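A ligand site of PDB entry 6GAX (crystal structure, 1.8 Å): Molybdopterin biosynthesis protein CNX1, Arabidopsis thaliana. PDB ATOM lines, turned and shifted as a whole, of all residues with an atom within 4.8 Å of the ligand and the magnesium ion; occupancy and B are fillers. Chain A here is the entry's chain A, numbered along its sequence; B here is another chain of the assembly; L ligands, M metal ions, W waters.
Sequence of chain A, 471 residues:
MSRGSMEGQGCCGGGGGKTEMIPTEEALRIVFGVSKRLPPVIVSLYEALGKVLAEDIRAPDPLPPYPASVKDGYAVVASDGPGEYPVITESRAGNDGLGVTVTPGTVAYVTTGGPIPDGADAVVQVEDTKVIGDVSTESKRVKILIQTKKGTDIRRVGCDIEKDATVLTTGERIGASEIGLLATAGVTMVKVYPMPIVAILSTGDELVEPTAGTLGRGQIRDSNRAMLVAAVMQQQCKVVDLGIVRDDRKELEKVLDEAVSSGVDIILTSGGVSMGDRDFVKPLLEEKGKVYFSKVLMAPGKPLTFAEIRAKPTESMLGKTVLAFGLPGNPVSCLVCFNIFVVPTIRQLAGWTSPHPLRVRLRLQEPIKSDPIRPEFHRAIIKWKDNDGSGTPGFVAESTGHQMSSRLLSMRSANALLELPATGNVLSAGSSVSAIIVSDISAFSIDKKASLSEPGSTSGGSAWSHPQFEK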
ATOM      1  N   SER A 202     -36.968   5.400  21.499  1.00  0.00           N
ATOM      2  CA  SER A 202     -35.639   5.282  20.900  1.00  0.00           C
ATOM      3  C   SER A 202     -34.934   6.589  21.141  1.00  0.00           C
ATOM      4  O   SER A 202     -35.584   7.625  21.344  1.00  0.00           O
ATOM      5  CB  SER A 202     -35.739   5.072  19.389  1.00  0.00           C
ATOM      6  OG  SER A 202     -36.109   3.726  19.178  1.00  0.00           O
ATOM      7  N   THR A 203     -33.610   6.558  21.126  1.00  0.00           N
ATOM      8  CA  THR A 203     -32.833   7.786  21.319  1.00  0.00           C
ATOM      9  C   THR A 203     -31.807   7.903  20.218  1.00  0.00           C
ATOM     10  O   THR A 203     -31.168   6.912  19.868  1.00  0.00           O
ATOM     11  CB  THR A 203     -32.092   7.834  22.699  1.00  0.00           C
ATOM     12  OG1 THR A 203     -31.003   6.898  22.716  1.00  0.00           O
ATOM     13  CG2 THR A 203     -33.003   7.610  23.911  1.00  0.00           C
ATOM     14  N   GLY A 204     -31.556   9.124  19.788  1.00  0.00           N
ATOM     15  CA  GLY A 204     -30.469   9.390  18.857  1.00  0.00           C
ATOM     16  C   GLY A 204     -30.725  10.483  17.847  1.00  0.00           C
ATOM     17  O   GLY A 204     -31.768  10.477  17.197  1.00  0.00           O
ATOM     18  N   GLU A 206     -29.106  10.577  15.102  1.00  0.00           N
ATOM     19  CA  GLU A 206     -28.932   9.921  13.802  1.00  0.00           C
ATOM     20  C   GLU A 206     -30.196   9.223  13.329  1.00  0.00           C
ATOM     21  O   GLU A 206     -30.269   8.870  12.161  1.00  0.00           O
ATOM     22  CB  GLU A 206     -27.739   8.899  13.808  1.00  0.00           C
ATOM     23  CG  GLU A 206     -27.975   7.545  14.464  1.00  0.00           C
ATOM     24  CD  GLU A 206     -27.965   7.506  15.986  1.00  0.00           C
ATOM     25  OE1 GLU A 206     -28.125   8.575  16.619  1.00  0.00           O
ATOM     26  OE2 GLU A 206     -27.798   6.404  16.547  1.00  0.00           O
ATOM     27  N   LEU A 207     -31.176   8.998  14.203  1.00  0.00           N
ATOM     28  CA  LEU A 207     -32.366   8.234  13.824  1.00  0.00           C
ATOM     29  C   LEU A 207     -33.365   9.000  13.016  1.00  0.00           C
ATOM     30  O   LEU A 207     -33.607  10.196  13.266  1.00  0.00           O
ATOM     31  CB  LEU A 207     -33.085   7.757  15.084  1.00  0.00           C
ATOM     32  CG  LEU A 207     -32.271   6.917  16.063  1.00  0.00           C
ATOM     33  CD1 LEU A 207     -33.179   6.499  17.226  1.00  0.00           C
ATOM     34  CD2 LEU A 207     -31.663   5.653  15.387  1.00  0.00           C
ATOM     35  N   ILE A 220     -29.913   6.849   9.964  1.00  0.00           N
ATOM     36  CA  ILE A 220     -30.334   5.455   9.878  1.00  0.00           C
ATOM     37  C   ILE A 220     -31.789   5.418  10.297  1.00  0.00           C
ATOM     38  O   ILE A 220     -32.236   6.256  11.098  1.00  0.00           O
ATOM     39  CB  ILE A 220     -29.495   4.469  10.749  1.00  0.00           C
ATOM     40  CG1 ILE A 220     -29.573   4.820  12.263  1.00  0.00           C
ATOM     41  CG2 ILE A 220     -28.029   4.451  10.271  1.00  0.00           C
ATOM     42  CD1 ILE A 220     -29.081   3.766  13.168  1.00  0.00           C
ATOM     43  N   ARG A 221     -32.515   4.410   9.814  1.00  0.00           N
ATOM     44  CA  ARG A 221     -33.897   4.229  10.265  1.00  0.00           C
ATOM     45  C   ARG A 221     -33.911   3.668  11.669  1.00  0.00           C
ATOM     46  O   ARG A 221     -33.084   2.802  12.003  1.00  0.00           O
ATOM     47  CB  ARG A 221     -34.666   3.279   9.351  1.00  0.00           C
ATOM     48  CG  ARG A 221     -34.851   3.912   7.962  1.00  0.00           C
ATOM     49  CD  ARG A 221     -35.729   3.113   7.007  1.00  0.00           C
ATOM     50  NE  ARG A 221     -35.567   3.679   5.656  1.00  0.00           N
ATOM     51  CZ  ARG A 221     -34.571   3.404   4.820  1.00  0.00           C
ATOM     52  NH1 ARG A 221     -33.666   2.480   5.130  1.00  0.00           N
ATOM     53  NH2 ARG A 221     -34.482   4.046   3.656  1.00  0.00           N
ATOM     54  N   ASP A 222     -34.842   4.158  12.497  1.00  0.00           N
ATOM     55  CA  ASP A 222     -35.035   3.646  13.846  1.00  0.00           C
ATOM     56  C   ASP A 222     -35.619   2.201  13.671  1.00  0.00           C
ATOM     57  O   ASP A 222     -36.745   2.041  13.223  1.00  0.00           O
ATOM     58  CB  ASP A 222     -36.075   4.545  14.579  1.00  0.00           C
ATOM     59  CG  ASP A 222     -36.509   4.085  15.966  1.00  0.00           C
ATOM     60  OD1 ASP A 222     -35.933   3.112  16.469  1.00  0.00           O
ATOM     61  OD2 ASP A 222     -37.381   4.744  16.558  1.00  0.00           O
ATOM     62  N   SER A 223     -34.826   1.180  13.971  1.00  0.00           N
ATOM     63  CA  SER A 223     -35.280  -0.214  13.900  1.00  0.00           C
ATOM     64  C   SER A 223     -35.594  -0.758  15.285  1.00  0.00           C
ATOM     65  O   SER A 223     -36.473  -1.617  15.407  1.00  0.00           O
ATOM     66  CB  SER A 223     -34.251  -1.103  13.197  1.00  0.00           C
ATOM     67  OG  SER A 223     -32.993  -1.155  13.836  1.00  0.00           O
ATOM     68  N   ASN A 224     -34.904  -0.279  16.337  1.00  0.00           N
ATOM     69  CA  ASN A 224     -35.140  -0.832  17.662  1.00  0.00           C
ATOM     70  C   ASN A 224     -36.547  -0.637  18.175  1.00  0.00           C
ATOM     71  O   ASN A 224     -37.034  -1.506  18.879  1.00  0.00           O
ATOM     72  CB  ASN A 224     -34.167  -0.232  18.694  1.00  0.00           C
ATOM     73  CG  ASN A 224     -32.749  -0.685  18.559  1.00  0.00           C
ATOM     74  OD1 ASN A 224     -32.421  -1.581  17.780  1.00  0.00           O
ATOM     75  ND2 ASN A 224     -31.860  -0.062  19.302  1.00  0.00           N
ATOM     76  N   ARG A 225     -37.163   0.523  17.938  1.00  0.00           N
ATOM     77  CA  ARG A 225     -38.479   0.793  18.502  1.00  0.00           C
ATOM     78  C   ARG A 225     -39.514  -0.165  17.938  1.00  0.00           C
ATOM     79  O   ARG A 225     -40.175  -0.839  18.703  1.00  0.00           O
ATOM     80  CB  ARG A 225     -38.886   2.271  18.292  1.00  0.00           C
ATOM     81  CG  ARG A 225     -40.205   2.701  18.946  1.00  0.00           C
ATOM     82  CD  ARG A 225     -40.223   4.220  19.093  1.00  0.00           C
ATOM     83  NE  ARG A 225     -39.795   4.846  17.838  1.00  0.00           N
ATOM     84  CZ  ARG A 225     -40.567   5.238  16.827  1.00  0.00           C
ATOM     85  NH1 ARG A 225     -41.887   5.223  16.938  1.00  0.00           N
ATOM     86  NH2 ARG A 225     -40.027   5.763  15.733  1.00  0.00           N
ATOM     87  N   ASP A 247     -30.737  13.417  21.392  1.00  0.00           N
ATOM     88  CA  ASP A 247     -29.690  13.384  22.410  1.00  0.00           C
ATOM     89  C   ASP A 247     -29.580  14.737  23.094  1.00  0.00           C
ATOM     90  O   ASP A 247     -28.590  15.436  22.962  1.00  0.00           O
ATOM     91  CB  ASP A 247     -28.336  12.922  21.782  1.00  0.00           C
ATOM     92  CG  ASP A 247     -28.458  11.555  21.146  1.00  0.00           C
ATOM     93  OD1 ASP A 247     -29.099  10.646  21.777  1.00  0.00           O
ATOM     94  OD2 ASP A 247     -27.972  11.387  20.020  1.00  0.00           O
ATOM     95  N   SER A 270     -33.752   2.622  24.274  1.00  0.00           N
ATOM     96  CA  SER A 270     -32.592   2.017  23.639  1.00  0.00           C
ATOM     97  C   SER A 270     -31.658   3.126  23.227  1.00  0.00           C
ATOM     98  O   SER A 270     -32.102   4.255  22.956  1.00  0.00           O
ATOM     99  CB  SER A 270     -32.934   1.075  22.489  1.00  0.00           C
ATOM    100  OG  SER A 270     -33.277   1.734  21.271  1.00  0.00           O
ATOM    101  N   GLY A 271     -30.362   2.853  23.265  1.00  0.00           N
ATOM    102  CA  GLY A 271     -29.353   3.852  22.928  1.00  0.00           C
ATOM    103  C   GLY A 271     -29.138   4.829  24.064  1.00  0.00           C
ATOM    104  O   GLY A 271     -29.784   4.711  25.105  1.00  0.00           O
ATOM    105  N   GLY A 272     -28.221   5.788  23.865  1.00  0.00           N
ATOM    106  CA  GLY A 272     -27.921   6.813  24.861  1.00  0.00           C
ATOM    107  C   GLY A 272     -27.395   6.293  26.194  1.00  0.00           C
ATOM    108  O   GLY A 272     -27.581   6.968  27.207  1.00  0.00           O
ATOM    109  N   VAL A 273     -26.786   5.087  26.204  1.00  0.00           N
ATOM    110  CA  VAL A 273     -26.300   4.419  27.427  1.00  0.00           C
ATOM    111  C   VAL A 273     -24.847   3.981  27.272  1.00  0.00           C
ATOM    112  O   VAL A 273     -24.432   3.176  28.072  1.00  0.00           O
ATOM    113  CB  VAL A 273     -27.147   3.163  27.860  1.00  0.00           C
ATOM    114  CG1 VAL A 273     -28.455   3.540  28.538  1.00  0.00           C
ATOM    115  CG2 VAL A 273     -27.390   2.213  26.709  1.00  0.00           C
ATOM    116  N   SER A 274     -24.091   4.439  26.254  1.00  0.00           N
ATOM    117  CA  SER A 274     -22.686   4.026  26.098  1.00  0.00           C
ATOM    118  C   SER A 274     -21.807   5.128  26.734  1.00  0.00           C
ATOM    119  O   SER A 274     -22.223   5.745  27.721  1.00  0.00           O
ATOM    120  CB  SER A 274     -22.341   3.805  24.617  1.00  0.00           C
ATOM    121  OG  SER A 274     -23.318   3.060  23.911  1.00  0.00           O
ATOM    122  N   ASP A 279     -24.956  10.870  25.952  1.00  0.00           N
ATOM    123  CA  ASP A 279     -25.679   9.654  26.378  1.00  0.00           C
ATOM    124  C   ASP A 279     -26.278  10.008  27.749  1.00  0.00           C
ATOM    125  O   ASP A 279     -25.569   9.984  28.734  1.00  0.00           O
ATOM    126  CB  ASP A 279     -24.676   8.465  26.448  1.00  0.00           C
ATOM    127  CG  ASP A 279     -24.344   7.879  25.075  1.00  0.00           C
ATOM    128  OD1 ASP A 279     -24.947   8.301  24.086  1.00  0.00           O
ATOM    129  OD2 ASP A 279     -23.480   6.988  25.013  1.00  0.00           O
ATOM    130  N   GLY A 329     -28.139   0.462  22.425  1.00  0.00           N
ATOM    131  CA  GLY A 329     -28.611   0.885  21.104  1.00  0.00           C
ATOM    132  C   GLY A 329     -28.332  -0.101  19.990  1.00  0.00           C
ATOM    133  O   GLY A 329     -29.084  -0.153  19.011  1.00  0.00           O
ATOM    134  N   ASN A 330     -27.247  -0.880  20.087  1.00  0.00           N
ATOM    135  CA  ASN A 330     -26.925  -1.846  19.026  1.00  0.00           C
ATOM    136  C   ASN A 330     -28.079  -2.830  18.884  1.00  0.00           C
ATOM    137  O   ASN A 330     -28.485  -3.416  19.884  1.00  0.00           O
ATOM    138  CB  ASN A 330     -25.625  -2.590  19.316  1.00  0.00           C
ATOM    139  CG  ASN A 330     -24.399  -1.819  18.891  1.00  0.00           C
ATOM    140  OD1 ASN A 330     -24.249  -1.416  17.736  1.00  0.00           O
ATOM    141  ND2 ASN A 330     -23.481  -1.621  19.806  1.00  0.00           N
ATOM    142  N   PRO A 331     -28.694  -2.937  17.683  1.00  0.00           N
ATOM    143  CA  PRO A 331     -29.917  -3.766  17.547  1.00  0.00           C
ATOM    144  C   PRO A 331     -29.875  -5.156  18.156  1.00  0.00           C
ATOM    145  O   PRO A 331     -30.841  -5.580  18.740  1.00  0.00           O
ATOM    146  CB  PRO A 331     -30.110  -3.845  16.031  1.00  0.00           C
ATOM    147  CG  PRO A 331     -29.572  -2.548  15.532  1.00  0.00           C
ATOM    148  CD  PRO A 331     -28.393  -2.223  16.418  1.00  0.00           C
ATOM    149  N   THR B 112     -20.549   6.512  19.304  1.00  0.00           N
ATOM    150  CA  THR B 112     -20.912   5.262  18.624  1.00  0.00           C
ATOM    151  C   THR B 112     -22.029   5.535  17.650  1.00  0.00           C
ATOM    152  O   THR B 112     -22.971   6.237  17.998  1.00  0.00           O
ATOM    153  CB  THR B 112     -21.333   4.186  19.642  1.00  0.00           C
ATOM    154  OG1 THR B 112     -20.312   4.071  20.625  1.00  0.00           O
ATOM    155  CG2 THR B 112     -21.569   2.836  18.985  1.00  0.00           C
ATOM    156  N   GLY B 113     -21.871   5.064  16.423  1.00  0.00           N
ATOM    157  CA  GLY B 113     -22.842   5.315  15.363  1.00  0.00           C
ATOM    158  C   GLY B 113     -22.591   6.628  14.623  1.00  0.00           C
ATOM    159  O   GLY B 113     -23.279   6.911  13.643  1.00  0.00           O
ATOM    160  N   ARG B 155     -17.381   0.623  11.290  1.00  0.00           N
ATOM    161  CA  ARG B 155     -18.274  -0.209  10.514  1.00  0.00           C
ATOM    162  C   ARG B 155     -18.265   0.430   9.120  1.00  0.00           C
ATOM    163  O   ARG B 155     -18.799   1.530   8.974  1.00  0.00           O
ATOM    164  CB  ARG B 155     -19.714  -0.167  11.077  1.00  0.00           C
ATOM    165  CG  ARG B 155     -19.866  -0.976  12.360  1.00  0.00           C
ATOM    166  CD  ARG B 155     -21.079  -0.571  13.176  1.00  0.00           C
ATOM    167  NE  ARG B 155     -22.318  -0.754  12.403  1.00  0.00           N
ATOM    168  CZ  ARG B 155     -23.340   0.100  12.349  1.00  0.00           C
ATOM    169  NH1 ARG B 155     -23.316   1.243  13.031  1.00  0.00           N
ATOM    170  NH2 ARG B 155     -24.394  -0.175  11.589  1.00  0.00           N
HETATM  171  P1  LIG L   1     -25.829   4.447  21.439  1.00  0.00           P
HETATM  172  O1  LIG L   1     -24.443   4.982  21.156  1.00  0.00           O
HETATM  173  O2  LIG L   1     -26.896   5.501  21.375  1.00  0.00           O
HETATM  174  O3  LIG L   1     -25.882   3.496  22.572  1.00  0.00           O
HETATM  175  O4  LIG L   1     -26.056   3.477  20.176  1.00  0.00           O
HETATM  176  C1  LIG L   1     -25.213   2.372  19.917  1.00  0.00           C
HETATM  177  C2  LIG L   1     -25.363   1.967  18.459  1.00  0.00           C
HETATM  178  O5  LIG L   1     -26.720   1.534  18.204  1.00  0.00           O
HETATM  179  C3  LIG L   1     -25.079   3.055  17.423  1.00  0.00           C
HETATM  180  O6  LIG L   1     -24.443   2.416  16.299  1.00  0.00           O
HETATM  181  C4  LIG L   1     -26.459   3.583  17.059  1.00  0.00           C
HETATM  182  O7  LIG L   1     -26.512   4.214  15.770  1.00  0.00           O
HETATM  183  C5  LIG L   1     -27.287   2.294  17.143  1.00  0.00           C
HETATM  184  N1  LIG L   1     -28.693   2.605  17.475  1.00  0.00           N
HETATM  185  C6  LIG L   1     -29.105   3.322  18.548  1.00  0.00           C
HETATM  186  N2  LIG L   1     -30.448   3.389  18.555  1.00  0.00           N
HETATM  187  C7  LIG L   1     -30.876   2.715  17.463  1.00  0.00           C
HETATM  188  C8  LIG L   1     -32.189   2.408  16.872  1.00  0.00           C
HETATM  189  N3  LIG L   1     -33.290   2.868  17.458  1.00  0.00           N
HETATM  190  N4  LIG L   1     -32.252   1.589  15.807  1.00  0.00           N
HETATM  191  C9  LIG L   1     -31.136   1.151  15.202  1.00  0.00           C
HETATM  192  N5  LIG L   1     -29.910   1.428  15.667  1.00  0.00           N
HETATM  193  C10 LIG L   1     -29.730   2.158  16.785  1.00  0.00           C
HETATM  194 MG    MG M   1     -27.122   7.183  20.389  1.00  0.00          MG
HETATM  195  O   HOH W   1     -21.992   1.726  15.511  1.00  0.00           O
HETATM  196  O   HOH W   2     -28.517   0.204  13.576  1.00  0.00           O
HETATM  197  O   HOH W   3     -25.223  -0.177  15.580  1.00  0.00           O
HETATM  198  O   HOH W   4     -28.627   6.329  19.090  1.00  0.00           O
HETATM  199  O   HOH W   5     -27.146   8.961  19.108  1.00  0.00           O
HETATM  200  O   HOH W   6     -22.909   6.718  22.394  1.00  0.00           O
HETATM  201  O   HOH W   7     -25.566   1.215  23.731  1.00  0.00           O
HETATM  202  O   HOH W   8     -28.643   7.909  21.655  1.00  0.00           O
HETATM  203  O   HOH W   9     -25.214   3.642  13.239  1.00  0.00           O
HETATM  204  O   HOH W  10     -25.563   8.152  21.469  1.00  0.00           O
HETATM  205  O   HOH W  11     -32.649   4.054  20.157  1.00  0.00           O
HETATM  206  O   HOH W  12     -25.744   6.703  18.798  1.00  0.00           O
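OE2 of Glu 206 lies within hydrogen-bond range of O7 of the ligand, 2.7 Å away. A nitrogen (N3) of the ligand lies within hydrogen-bond range of the side-chain carboxylate (OD1) of Asp 222 (2.8 Å). N of Gly 272 lies close to O2 of the ligand (2.8 Å). The side-chain hydroxyl (OG) of Ser 274 sits at hydrogen-bond distance from an oxygen (O3) of the ligand (2.9 Å). The backbone NH of Asn 330 lies within hydrogen-bond range of an oxygen (O5) of the ligand (3.1 Å). N of Ser 223 is in hydrogen-bond range of N4 of the ligand (3.2 Å). The side-chain hydroxyl (OG) of Ser 223 sits close to a nitrogen (N4) of the ligand (3.5 Å). The backbone NH of Asn 224 lies within hydrogen-bond range of a nitrogen (N4) of the ligand (3.3 Å). The side-chain hydroxyl of Ser 202 is in hydrogen-bond range of a nitrogen (N3) of the ligand, at 3.4 Å.
O of Glu 206 lies within hydrogen-bond range of N of Ile 220 (3.0 Å). OG of Ser 202 is in hydrogen-bond range of OD1 of Asp 222, at 2.8 Å. The guanidinium group of Arg 225 lies within salt-bridge range of the side-chain carboxylate of Asp 222. The backbone NH (N) of Gly 272 is in hydrogen-bond range of the side-chain hydroxyl (OG1) of Thr 203, at 3.2 Å. ND2 of Asn 224 lies within hydrogen-bond range of O of Gly 329. N of Ser 274 is in hydrogen-bond range of OD2 of Asp 279, 2.9 Å away. The side-chain amide nitrogen (ND2) of Asn 224 sits at hydrogen-bond distance from the side-chain hydroxyl (OG) of Ser 270 (3.0 Å). The backbone carbonyl oxygen (O) of Gly 271 sits close to the side-chain hydroxyl (OG1) of Thr 203.
The backbone carbonyl oxygen (O) of Gly 329 lies close to an oxygen (O5) of the ligand. Residues that only touch the ligand: Thr 203, Leu 207, Ile 220, Ser 270, Gly 271, Pro 331, Thr 112 of chain B, Gly 113 of chain B and Arg 155 of chain B. Within 4 Å of the ligand: Ser 202, Thr 203, Glu 206, Leu 207, Ile 220, Asp 222, Ser 223, Asn 224, Ser 270, Gly 271, Gly 272, Ser 274, Gly 329, Asn 330, Pro 331, Thr 112 of chain B, Gly 113 of chain B and Arg 155 of chain B.
Residues that only touch the magnesium ion: Glu 206 (3.98 Å) and Gly 272 (3.9 Å). Of the 24 residues printed, 2 come within 4 Å of the magnesium ion.
The magnesium ion is bound by O2 of the ligand (2.0 Å), water W8 (2.1 Å), water W10 (2.1 Å), water W12 (2.2 Å), water W4 (2.2 Å) and water W5 (2.2 Å). The magnesium ion has six donor atoms within binding distance.
Water W8 lies within hydrogen-bond range of OD1 of Asp 247 (2.8 Å), OG1 of Thr 203 (2.8 Å) and N of Gly 272 (3.1 Å). Water W5 lies within hydrogen-bond range of the side-chain carboxylate (OE1) of Glu 206 and the side-chain carboxylate (OD2) of Asp 247. Water W7 lies within hydrogen-bond range of an oxygen (O3) of the ligand (2.6 Å), the side-chain hydroxyl of Ser 274 (2.9 Å) and the backbone NH of Gly 329 (3.0 Å). Water W1 lies within hydrogen-bond range of O6 of the ligand (2.7 Å), NH1 of Arg 155 of chain B (2.9 Å) and N of Gly 113 of chain B (3.5 Å). Water W3 lies within hydrogen-bond range of the side-chain amide oxygen of Asn 330, an oxygen (O6) of the ligand and the guanidinium group of Arg 155 of chain B. Water W11 lies within hydrogen-bond range of OG of Ser 270 (2.6 Å), N2 of the ligand (2.8 Å) and N of Thr 203 (2.9 Å).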
